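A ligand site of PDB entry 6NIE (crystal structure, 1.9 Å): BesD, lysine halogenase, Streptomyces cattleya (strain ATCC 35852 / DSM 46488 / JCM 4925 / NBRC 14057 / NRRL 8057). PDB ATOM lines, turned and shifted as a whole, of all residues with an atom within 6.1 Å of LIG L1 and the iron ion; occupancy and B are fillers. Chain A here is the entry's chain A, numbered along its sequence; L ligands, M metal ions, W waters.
The side-chain hydroxyl of Tyr 198 sits at hydrogen-bond distance from an oxygen (O4) of LIG L1, at 2.6 Å.
The guanidinium group of Arg 218 lies within salt-bridge range of an oxygen (O5) of LIG L1.
The side-chain amide nitrogen (ND2) of Asn 222 sits at hydrogen-bond distance from an oxygen (O2) of LIG L1, 2.7 Å away.
O1 of LG3 L3 sits at hydrogen-bond distance from NE2 of His 137, at 2.7 Å.
The backbone carbonyl oxygen (O) of Trp 141 lies within hydrogen-bond range of a nitrogen (N1) of LG3 L3 (2.9 Å).
A ring nitrogen (NE2) of His 140 sits close to a ring nitrogen (NE2) of His 137 (3.5 Å).
The backbone carbonyl oxygen (O) of Tyr 198 is in hydrogen-bond range of the backbone NH (N) of Ile 149, 2.7 Å away.
O of Arg 218 sits at hydrogen-bond distance from N of Gln 130, 2.7 Å away.
The guanidinium group (NE) of Arg 218 sits at hydrogen-bond distance from the backbone carbonyl oxygen (O) of Gly 161 (2.8 Å).
N of Asn 222 sits at hydrogen-bond distance from O of Leu 126.
The side-chain hydroxyl (OG1) of Thr 209 lies within hydrogen-bond range of the backbone NH (N) of His 137.
The side-chain hydroxyl (OG1) of Thr 209 is in hydrogen-bond range of the side-chain amide nitrogen (NE2) of Gln 130.
The backbone NH (N) of Ile 220 sits at hydrogen-bond distance from the backbone carbonyl oxygen (O) of Thr 128.
His 137 touches LIG L1 (CE1 to C2, 3.6 Å).
CG2 of Ile 149 touches O4 of LIG L1, 3.8 Å away.
Thr 209 touches LIG L1.
CG1 of Ile 220 touches O5 of LIG L1, 3.7 Å away.
Hydrophobic or aromatic side chains that line LIG L1: His 137, His 140, Ile 149, Tyr 198, His 207 and Ile 220.
Within 4 Å of LIG L1: His 137, His 140, Ile 149, Tyr 198, His 207, Thr 209, Arg 218, Ile 220 and Asn 222.
Along chain A the residues within 4 Å of LIG L1 span positions 137 to 222.
The nearest printed residue that does not touch LIG L1 is Leu 163 (4.2 Å).
Two residues have an atom within 4 Å of the iron ion: His 140 and His 207.
O1 of LIG L1 binds the iron ion (2.2 Å).
An oxygen (O3) of LIG L1 is bound to the iron ion, 2.2 Å away.
NE2 of His 207 binds the iron ion, 2.2 Å away.
The iron ion is bound by NE2 of His 140.
The iron ion is bound by CL1 of LG2 L2, 2.4 Å away.
Water W1 lies within hydrogen-bond range of an oxygen (O5) of LIG L1 (2.8 Å), the side-chain hydroxyl (OG1) of Thr 128 (2.8 Å), a ring nitrogen (ND1) of His 137 (2.9 Å) and the side-chain amide nitrogen (NE2) of Gln 130 (3.3 Å).
Water W2 bridges N2 of LG3 L3 (2.8 Å) and ND2 of Asn 222 (2.9 Å).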
ATOM      1  N   LEU A 126      28.602   7.930 -16.875  1.00  0.00           N
ATOM      2  CA  LEU A 126      28.213   8.721 -15.721  1.00  0.00           C
ATOM      3  C   LEU A 126      26.772   8.390 -15.381  1.00  0.00           C
ATOM      4  O   LEU A 126      25.916   8.390 -16.269  1.00  0.00           O
ATOM      5  CB  LEU A 126      28.365  10.227 -15.984  1.00  0.00           C
ATOM      6  CG  LEU A 126      27.971  11.233 -14.876  1.00  0.00           C
ATOM      7  CD1 LEU A 126      28.934  11.101 -13.715  1.00  0.00           C
ATOM      8  CD2 LEU A 126      27.966  12.606 -15.409  1.00  0.00           C
ATOM      9  N   THR A 128      23.704  10.016 -13.152  1.00  0.00           N
ATOM     10  CA  THR A 128      23.287  11.118 -12.288  1.00  0.00           C
ATOM     11  C   THR A 128      21.899  10.852 -11.711  1.00  0.00           C
ATOM     12  O   THR A 128      21.043  10.211 -12.336  1.00  0.00           O
ATOM     13  CB  THR A 128      23.264  12.479 -12.997  1.00  0.00           C
ATOM     14  OG1 THR A 128      22.203  12.518 -13.956  1.00  0.00           O
ATOM     15  CG2 THR A 128      24.595  12.774 -13.709  1.00  0.00           C
ATOM     16  N   GLN A 130      19.051  13.247  -9.811  1.00  0.00           N
ATOM     17  CA  GLN A 130      18.518  14.443  -9.204  1.00  0.00           C
ATOM     18  C   GLN A 130      17.383  14.064  -8.263  1.00  0.00           C
ATOM     19  O   GLN A 130      16.539  13.222  -8.585  1.00  0.00           O
ATOM     20  CB  GLN A 130      18.079  15.423 -10.287  1.00  0.00           C
ATOM     21  CG  GLN A 130      19.240  15.636 -11.259  1.00  0.00           C
ATOM     22  CD  GLN A 130      18.913  16.601 -12.360  1.00  0.00           C
ATOM     23  OE1 GLN A 130      18.145  17.539 -12.145  1.00  0.00           O
ATOM     24  NE2 GLN A 130      19.503  16.397 -13.526  1.00  0.00           N
ATOM     25  N   HIS A 137      20.918  19.903 -13.938  1.00  0.00           N
ATOM     26  CA  HIS A 137      22.171  19.779 -14.675  1.00  0.00           C
ATOM     27  C   HIS A 137      22.243  21.034 -15.544  1.00  0.00           C
ATOM     28  O   HIS A 137      21.648  21.087 -16.627  1.00  0.00           O
ATOM     29  CB  HIS A 137      22.194  18.474 -15.484  1.00  0.00           C
ATOM     30  CG  HIS A 137      23.569  18.044 -15.886  1.00  0.00           C
ATOM     31  ND1 HIS A 137      23.921  16.715 -16.021  1.00  0.00           N
ATOM     32  CD2 HIS A 137      24.684  18.759 -16.175  1.00  0.00           C
ATOM     33  CE1 HIS A 137      25.191  16.639 -16.386  1.00  0.00           C
ATOM     34  NE2 HIS A 137      25.670  17.857 -16.512  1.00  0.00           N
ATOM     35  N   HIS A 140      25.361  23.575 -20.358  1.00  0.00           N
ATOM     36  CA  HIS A 140      26.718  23.112 -20.656  1.00  0.00           C
ATOM     37  C   HIS A 140      26.767  22.437 -22.017  1.00  0.00           C
ATOM     38  O   HIS A 140      25.742  22.165 -22.645  1.00  0.00           O
ATOM     39  CB  HIS A 140      27.205  22.135 -19.600  1.00  0.00           C
ATOM     40  CG  HIS A 140      26.434  20.858 -19.606  1.00  0.00           C
ATOM     41  ND1 HIS A 140      25.244  20.720 -18.912  1.00  0.00           N
ATOM     42  CD2 HIS A 140      26.670  19.659 -20.186  1.00  0.00           C
ATOM     43  CE1 HIS A 140      24.759  19.513 -19.116  1.00  0.00           C
ATOM     44  NE2 HIS A 140      25.632  18.833 -19.841  1.00  0.00           N
ATOM     45  N   TRP A 141      27.983  22.163 -22.465  1.00  0.00           N
ATOM     46  CA  TRP A 141      28.283  21.274 -23.582  1.00  0.00           C
ATOM     47  C   TRP A 141      29.131  20.104 -23.077  1.00  0.00           C
ATOM     48  O   TRP A 141      29.535  20.061 -21.916  1.00  0.00           O
ATOM     49  CB  TRP A 141      29.070  22.009 -24.675  1.00  0.00           C
ATOM     50  CG  TRP A 141      28.410  23.168 -25.342  1.00  0.00           C
ATOM     51  CD1 TRP A 141      27.765  23.152 -26.531  1.00  0.00           C
ATOM     52  CD2 TRP A 141      28.393  24.536 -24.884  1.00  0.00           C
ATOM     53  NE1 TRP A 141      27.352  24.403 -26.866  1.00  0.00           N
ATOM     54  CE2 TRP A 141      27.700  25.277 -25.866  1.00  0.00           C
ATOM     55  CE3 TRP A 141      28.874  25.202 -23.748  1.00  0.00           C
ATOM     56  CZ2 TRP A 141      27.510  26.665 -25.766  1.00  0.00           C
ATOM     57  CZ3 TRP A 141      28.660  26.602 -23.633  1.00  0.00           C
ATOM     58  CH2 TRP A 141      27.972  27.305 -24.648  1.00  0.00           C
ATOM     59  N   GLY A 142      29.438  19.165 -23.983  1.00  0.00           N
ATOM     60  CA  GLY A 142      30.357  18.077 -23.724  1.00  0.00           C
ATOM     61  C   GLY A 142      31.706  18.285 -24.369  1.00  0.00           C
ATOM     62  O   GLY A 142      31.827  18.920 -25.412  1.00  0.00           O
ATOM     63  N   ALA A 147      26.713  11.295 -26.756  1.00  0.00           N
ATOM     64  CA  ALA A 147      26.273  10.627 -25.538  1.00  0.00           C
ATOM     65  C   ALA A 147      24.970   9.894 -25.832  1.00  0.00           C
ATOM     66  O   ALA A 147      24.090  10.414 -26.532  1.00  0.00           O
ATOM     67  CB  ALA A 147      26.087  11.606 -24.365  1.00  0.00           C
ATOM     68  N   ILE A 149      21.926   8.666 -23.680  1.00  0.00           N
ATOM     69  CA  ILE A 149      21.372   8.972 -22.372  1.00  0.00           C
ATOM     70  C   ILE A 149      20.203   8.038 -22.137  1.00  0.00           C
ATOM     71  O   ILE A 149      19.203   8.113 -22.852  1.00  0.00           O
ATOM     72  CB  ILE A 149      20.891  10.442 -22.265  1.00  0.00           C
ATOM     73  CG1 ILE A 149      22.007  11.437 -22.590  1.00  0.00           C
ATOM     74  CG2 ILE A 149      20.373  10.688 -20.850  1.00  0.00           C
ATOM     75  CD1 ILE A 149      23.254  11.279 -21.694  1.00  0.00           C
ATOM     76  N   VAL A 151      17.271   7.337 -19.840  1.00  0.00           N
ATOM     77  CA  VAL A 151      16.416   7.959 -18.839  1.00  0.00           C
ATOM     78  C   VAL A 151      15.785   6.833 -18.028  1.00  0.00           C
ATOM     79  O   VAL A 151      14.754   6.283 -18.398  1.00  0.00           O
ATOM     80  CB  VAL A 151      15.349   8.855 -19.494  1.00  0.00           C
ATOM     81  CG1 VAL A 151      14.509   9.521 -18.413  1.00  0.00           C
ATOM     82  CG2 VAL A 151      16.040   9.864 -20.395  1.00  0.00           C
ATOM     83  N   GLY A 161      12.719  18.672 -14.730  1.00  0.00           N
ATOM     84  CA  GLY A 161      13.676  17.688 -15.196  1.00  0.00           C
ATOM     85  C   GLY A 161      13.687  17.506 -16.684  1.00  0.00           C
ATOM     86  O   GLY A 161      14.317  16.563 -17.184  1.00  0.00           O
ATOM     87  N   LEU A 163      14.682  18.159 -20.585  1.00  0.00           N
ATOM     88  CA  LEU A 163      15.896  18.575 -21.267  1.00  0.00           C
ATOM     89  C   LEU A 163      15.619  19.760 -22.192  1.00  0.00           C
ATOM     90  O   LEU A 163      14.626  19.767 -22.920  1.00  0.00           O
ATOM     91  CB  LEU A 163      16.471  17.412 -22.083  1.00  0.00           C
ATOM     92  CG  LEU A 163      17.865  17.595 -22.690  1.00  0.00           C
ATOM     93  CD1 LEU A 163      18.957  17.533 -21.592  1.00  0.00           C
ATOM     94  CD2 LEU A 163      18.109  16.472 -23.703  1.00  0.00           C
ATOM     95  N   PHE A 192      11.144  13.527 -21.347  1.00  0.00           N
ATOM     96  CA  PHE A 192      11.403  12.093 -21.486  1.00  0.00           C
ATOM     97  C   PHE A 192      10.750  11.342 -20.340  1.00  0.00           C
ATOM     98  O   PHE A 192      10.713  11.839 -19.209  1.00  0.00           O
ATOM     99  CB  PHE A 192      12.888  11.823 -21.557  1.00  0.00           C
ATOM    100  CG  PHE A 192      13.530  12.376 -22.798  1.00  0.00           C
ATOM    101  CD1 PHE A 192      13.329  11.744 -24.010  1.00  0.00           C
ATOM    102  CD2 PHE A 192      14.316  13.515 -22.741  1.00  0.00           C
ATOM    103  CE1 PHE A 192      13.923  12.255 -25.168  1.00  0.00           C
ATOM    104  CE2 PHE A 192      14.905  14.024 -23.886  1.00  0.00           C
ATOM    105  CZ  PHE A 192      14.713  13.411 -25.085  1.00  0.00           C
ATOM    106  N   TYR A 198      17.834   8.478 -25.345  1.00  0.00           N
ATOM    107  CA  TYR A 198      18.052   9.431 -26.412  1.00  0.00           C
ATOM    108  C   TYR A 198      19.540   9.573 -26.694  1.00  0.00           C
ATOM    109  O   TYR A 198      20.410   9.255 -25.860  1.00  0.00           O
ATOM    110  CB  TYR A 198      17.385  10.823 -26.112  1.00  0.00           C
ATOM    111  CG  TYR A 198      17.975  11.652 -24.974  1.00  0.00           C
ATOM    112  CD1 TYR A 198      19.058  12.511 -25.191  1.00  0.00           C
ATOM    113  CD2 TYR A 198      17.428  11.600 -23.706  1.00  0.00           C
ATOM    114  CE1 TYR A 198      19.585  13.285 -24.169  1.00  0.00           C
ATOM    115  CE2 TYR A 198      17.941  12.382 -22.650  1.00  0.00           C
ATOM    116  CZ  TYR A 198      19.034  13.210 -22.881  1.00  0.00           C
ATOM    117  OH  TYR A 198      19.559  13.985 -21.838  1.00  0.00           O
ATOM    118  N   LEU A 200      22.462  12.130 -28.190  1.00  0.00           N
ATOM    119  CA  LEU A 200      22.710  13.560 -28.140  1.00  0.00           C
ATOM    120  C   LEU A 200      24.077  13.883 -28.718  1.00  0.00           C
ATOM    121  O   LEU A 200      25.086  13.284 -28.328  1.00  0.00           O
ATOM    122  CB  LEU A 200      22.655  14.052 -26.695  1.00  0.00           C
ATOM    123  CG  LEU A 200      22.847  15.541 -26.384  1.00  0.00           C
ATOM    124  CD1 LEU A 200      21.742  16.433 -27.069  1.00  0.00           C
ATOM    125  CD2 LEU A 200      22.761  15.666 -24.886  1.00  0.00           C
ATOM    126  N   THR A 202      26.763  16.081 -28.174  1.00  0.00           N
ATOM    127  CA  THR A 202      26.966  16.903 -26.970  1.00  0.00           C
ATOM    128  C   THR A 202      27.961  18.031 -27.160  1.00  0.00           C
ATOM    129  O   THR A 202      27.895  19.037 -26.426  1.00  0.00           O
ATOM    130  CB  THR A 202      27.415  16.023 -25.803  1.00  0.00           C
ATOM    131  OG1 THR A 202      28.348  15.045 -26.285  1.00  0.00           O
ATOM    132  CG2 THR A 202      26.204  15.325 -25.205  1.00  0.00           C
ATOM    133  N   HIS A 207      22.962  22.308 -23.691  1.00  0.00           N
ATOM    134  CA  HIS A 207      21.805  21.667 -23.096  1.00  0.00           C
ATOM    135  C   HIS A 207      21.866  21.742 -21.583  1.00  0.00           C
ATOM    136  O   HIS A 207      22.922  21.994 -20.992  1.00  0.00           O
ATOM    137  CB  HIS A 207      21.649  20.189 -23.575  1.00  0.00           C
ATOM    138  CG  HIS A 207      22.879  19.351 -23.339  1.00  0.00           C
ATOM    139  ND1 HIS A 207      24.028  19.478 -24.104  1.00  0.00           N
ATOM    140  CD2 HIS A 207      23.160  18.419 -22.399  1.00  0.00           C
ATOM    141  CE1 HIS A 207      24.952  18.645 -23.645  1.00  0.00           C
ATOM    142  NE2 HIS A 207      24.443  17.990 -22.631  1.00  0.00           N
ATOM    143  N   ARG A 208      20.708  21.485 -20.959  1.00  0.00           N
ATOM    144  CA  ARG A 208      20.559  21.480 -19.510  1.00  0.00           C
ATOM    145  C   ARG A 208      19.323  20.663 -19.151  1.00  0.00           C
ATOM    146  O   ARG A 208      18.550  20.243 -20.016  1.00  0.00           O
ATOM    147  CB  ARG A 208      20.410  22.910 -18.944  1.00  0.00           C
ATOM    148  CG  ARG A 208      19.001  23.525 -19.217  1.00  0.00           C
ATOM    149  CD  ARG A 208      18.666  24.650 -18.209  1.00  0.00           C
ATOM    150  NE  ARG A 208      17.342  25.243 -18.512  1.00  0.00           N
ATOM    151  CZ  ARG A 208      16.637  25.918 -17.628  1.00  0.00           C
ATOM    152  NH1 ARG A 208      17.129  26.090 -16.422  1.00  0.00           N
ATOM    153  NH2 ARG A 208      15.448  26.446 -17.984  1.00  0.00           N
ATOM    154  N   THR A 209      19.150  20.434 -17.852  1.00  0.00           N
ATOM    155  CA  THR A 209      17.861  19.956 -17.367  1.00  0.00           C
ATOM    156  C   THR A 209      17.192  21.080 -16.586  1.00  0.00           C
ATOM    157  O   THR A 209      17.871  21.838 -15.858  1.00  0.00           O
ATOM    158  CB  THR A 209      17.966  18.691 -16.506  1.00  0.00           C
ATOM    159  OG1 THR A 209      18.644  18.994 -15.279  1.00  0.00           O
ATOM    160  CG2 THR A 209      18.686  17.577 -17.273  1.00  0.00           C
ATOM    161  N   ARG A 218      15.110  11.559 -10.356  1.00  0.00           N
ATOM    162  CA  ARG A 218      15.417  11.547 -11.782  1.00  0.00           C
ATOM    163  C   ARG A 218      16.803  10.927 -11.971  1.00  0.00           C
ATOM    164  O   ARG A 218      17.792  11.439 -11.422  1.00  0.00           O
ATOM    165  CB  ARG A 218      15.335  12.957 -12.380  1.00  0.00           C
ATOM    166  CG  ARG A 218      15.470  12.982 -13.886  1.00  0.00           C
ATOM    167  CD  ARG A 218      15.597  14.399 -14.429  1.00  0.00           C
ATOM    168  NE  ARG A 218      15.683  14.432 -15.901  1.00  0.00           N
ATOM    169  CZ  ARG A 218      16.799  14.217 -16.589  1.00  0.00           C
ATOM    170  NH1 ARG A 218      17.929  13.913 -15.971  1.00  0.00           N
ATOM    171  NH2 ARG A 218      16.769  14.258 -17.907  1.00  0.00           N
ATOM    172  N   ILE A 220      19.567   9.151 -14.792  1.00  0.00           N
ATOM    173  CA  ILE A 220      19.999   8.823 -16.143  1.00  0.00           C
ATOM    174  C   ILE A 220      21.336   8.091 -16.051  1.00  0.00           C
ATOM    175  O   ILE A 220      22.079   8.200 -15.065  1.00  0.00           O
ATOM    176  CB  ILE A 220      20.129  10.075 -17.049  1.00  0.00           C
ATOM    177  CG1 ILE A 220      21.249  10.996 -16.531  1.00  0.00           C
ATOM    178  CG2 ILE A 220      18.776  10.828 -17.176  1.00  0.00           C
ATOM    179  CD1 ILE A 220      22.600  10.796 -17.230  1.00  0.00           C
ATOM    180  N   ASN A 222      24.680   7.919 -18.628  1.00  0.00           N
ATOM    181  CA  ASN A 222      25.305   8.557 -19.783  1.00  0.00           C
ATOM    182  C   ASN A 222      26.458   7.652 -20.214  1.00  0.00           C
ATOM    183  O   ASN A 222      27.344   7.328 -19.405  1.00  0.00           O
ATOM    184  CB  ASN A 222      25.785   9.961 -19.412  1.00  0.00           C
ATOM    185  CG  ASN A 222      26.532  10.679 -20.531  1.00  0.00           C
ATOM    186  OD1 ASN A 222      27.236  10.063 -21.323  1.00  0.00           O
ATOM    187  ND2 ASN A 222      26.427  12.011 -20.549  1.00  0.00           N
HETATM  188  C1  LIG L   1      24.897  14.601 -19.422  1.00  0.00           C
HETATM  189  O1  LIG L   1      25.925  15.106 -19.901  1.00  0.00           O
HETATM  190  O2  LIG L   1      24.822  13.464 -18.887  1.00  0.00           O
HETATM  191  C2  LIG L   1      23.672  15.401 -19.439  1.00  0.00           C
HETATM  192  O3  LIG L   1      23.670  16.496 -19.926  1.00  0.00           O
HETATM  193  C3  LIG L   1      22.490  14.791 -18.758  1.00  0.00           C
HETATM  194  C4  LIG L   1      21.275  14.671 -19.574  1.00  0.00           C
HETATM  195  C5  LIG L   1      20.025  14.302 -18.732  1.00  0.00           C
HETATM  196  O4  LIG L   1      19.001  13.901 -19.351  1.00  0.00           O
HETATM  197  O5  LIG L   1      20.075  14.396 -17.475  1.00  0.00           O
HETATM  198 CL1  LG2 L   2      27.640  16.875 -22.096  1.00  0.00          CL
HETATM  199  N1  LG3 L   3      30.470  18.548 -19.685  1.00  0.00           N
HETATM  200  C1  LG3 L   3      29.415  18.097 -18.766  1.00  0.00           C
HETATM  201  C2  LG3 L   3      29.048  19.179 -17.746  1.00  0.00           C
HETATM  202  O1  LG3 L   3      28.121  19.022 -16.918  1.00  0.00           O
HETATM  203  C3  LG3 L   3      29.829  16.804 -18.045  1.00  0.00           C
HETATM  204  C4  LG3 L   3      29.596  15.502 -18.887  1.00  0.00           C
HETATM  205  C5  LG3 L   3      30.091  14.242 -18.114  1.00  0.00           C
HETATM  206  C6  LG3 L   3      29.575  12.923 -18.742  1.00  0.00           C
HETATM  207  N2  LG3 L   3      30.029  12.763 -20.187  1.00  0.00           N
HETATM  208  O2  LG3 L   3      29.638  20.248 -17.738  1.00  0.00           O
HETATM  209 FE    FE M   1      25.517  16.920 -21.012  1.00  0.00          FE
HETATM  210  O   HOH W   1      21.783  14.917 -15.341  1.00  0.00           O
HETATM  211  O   HOH W   2      28.221  13.810 -22.011  1.00  0.00           O
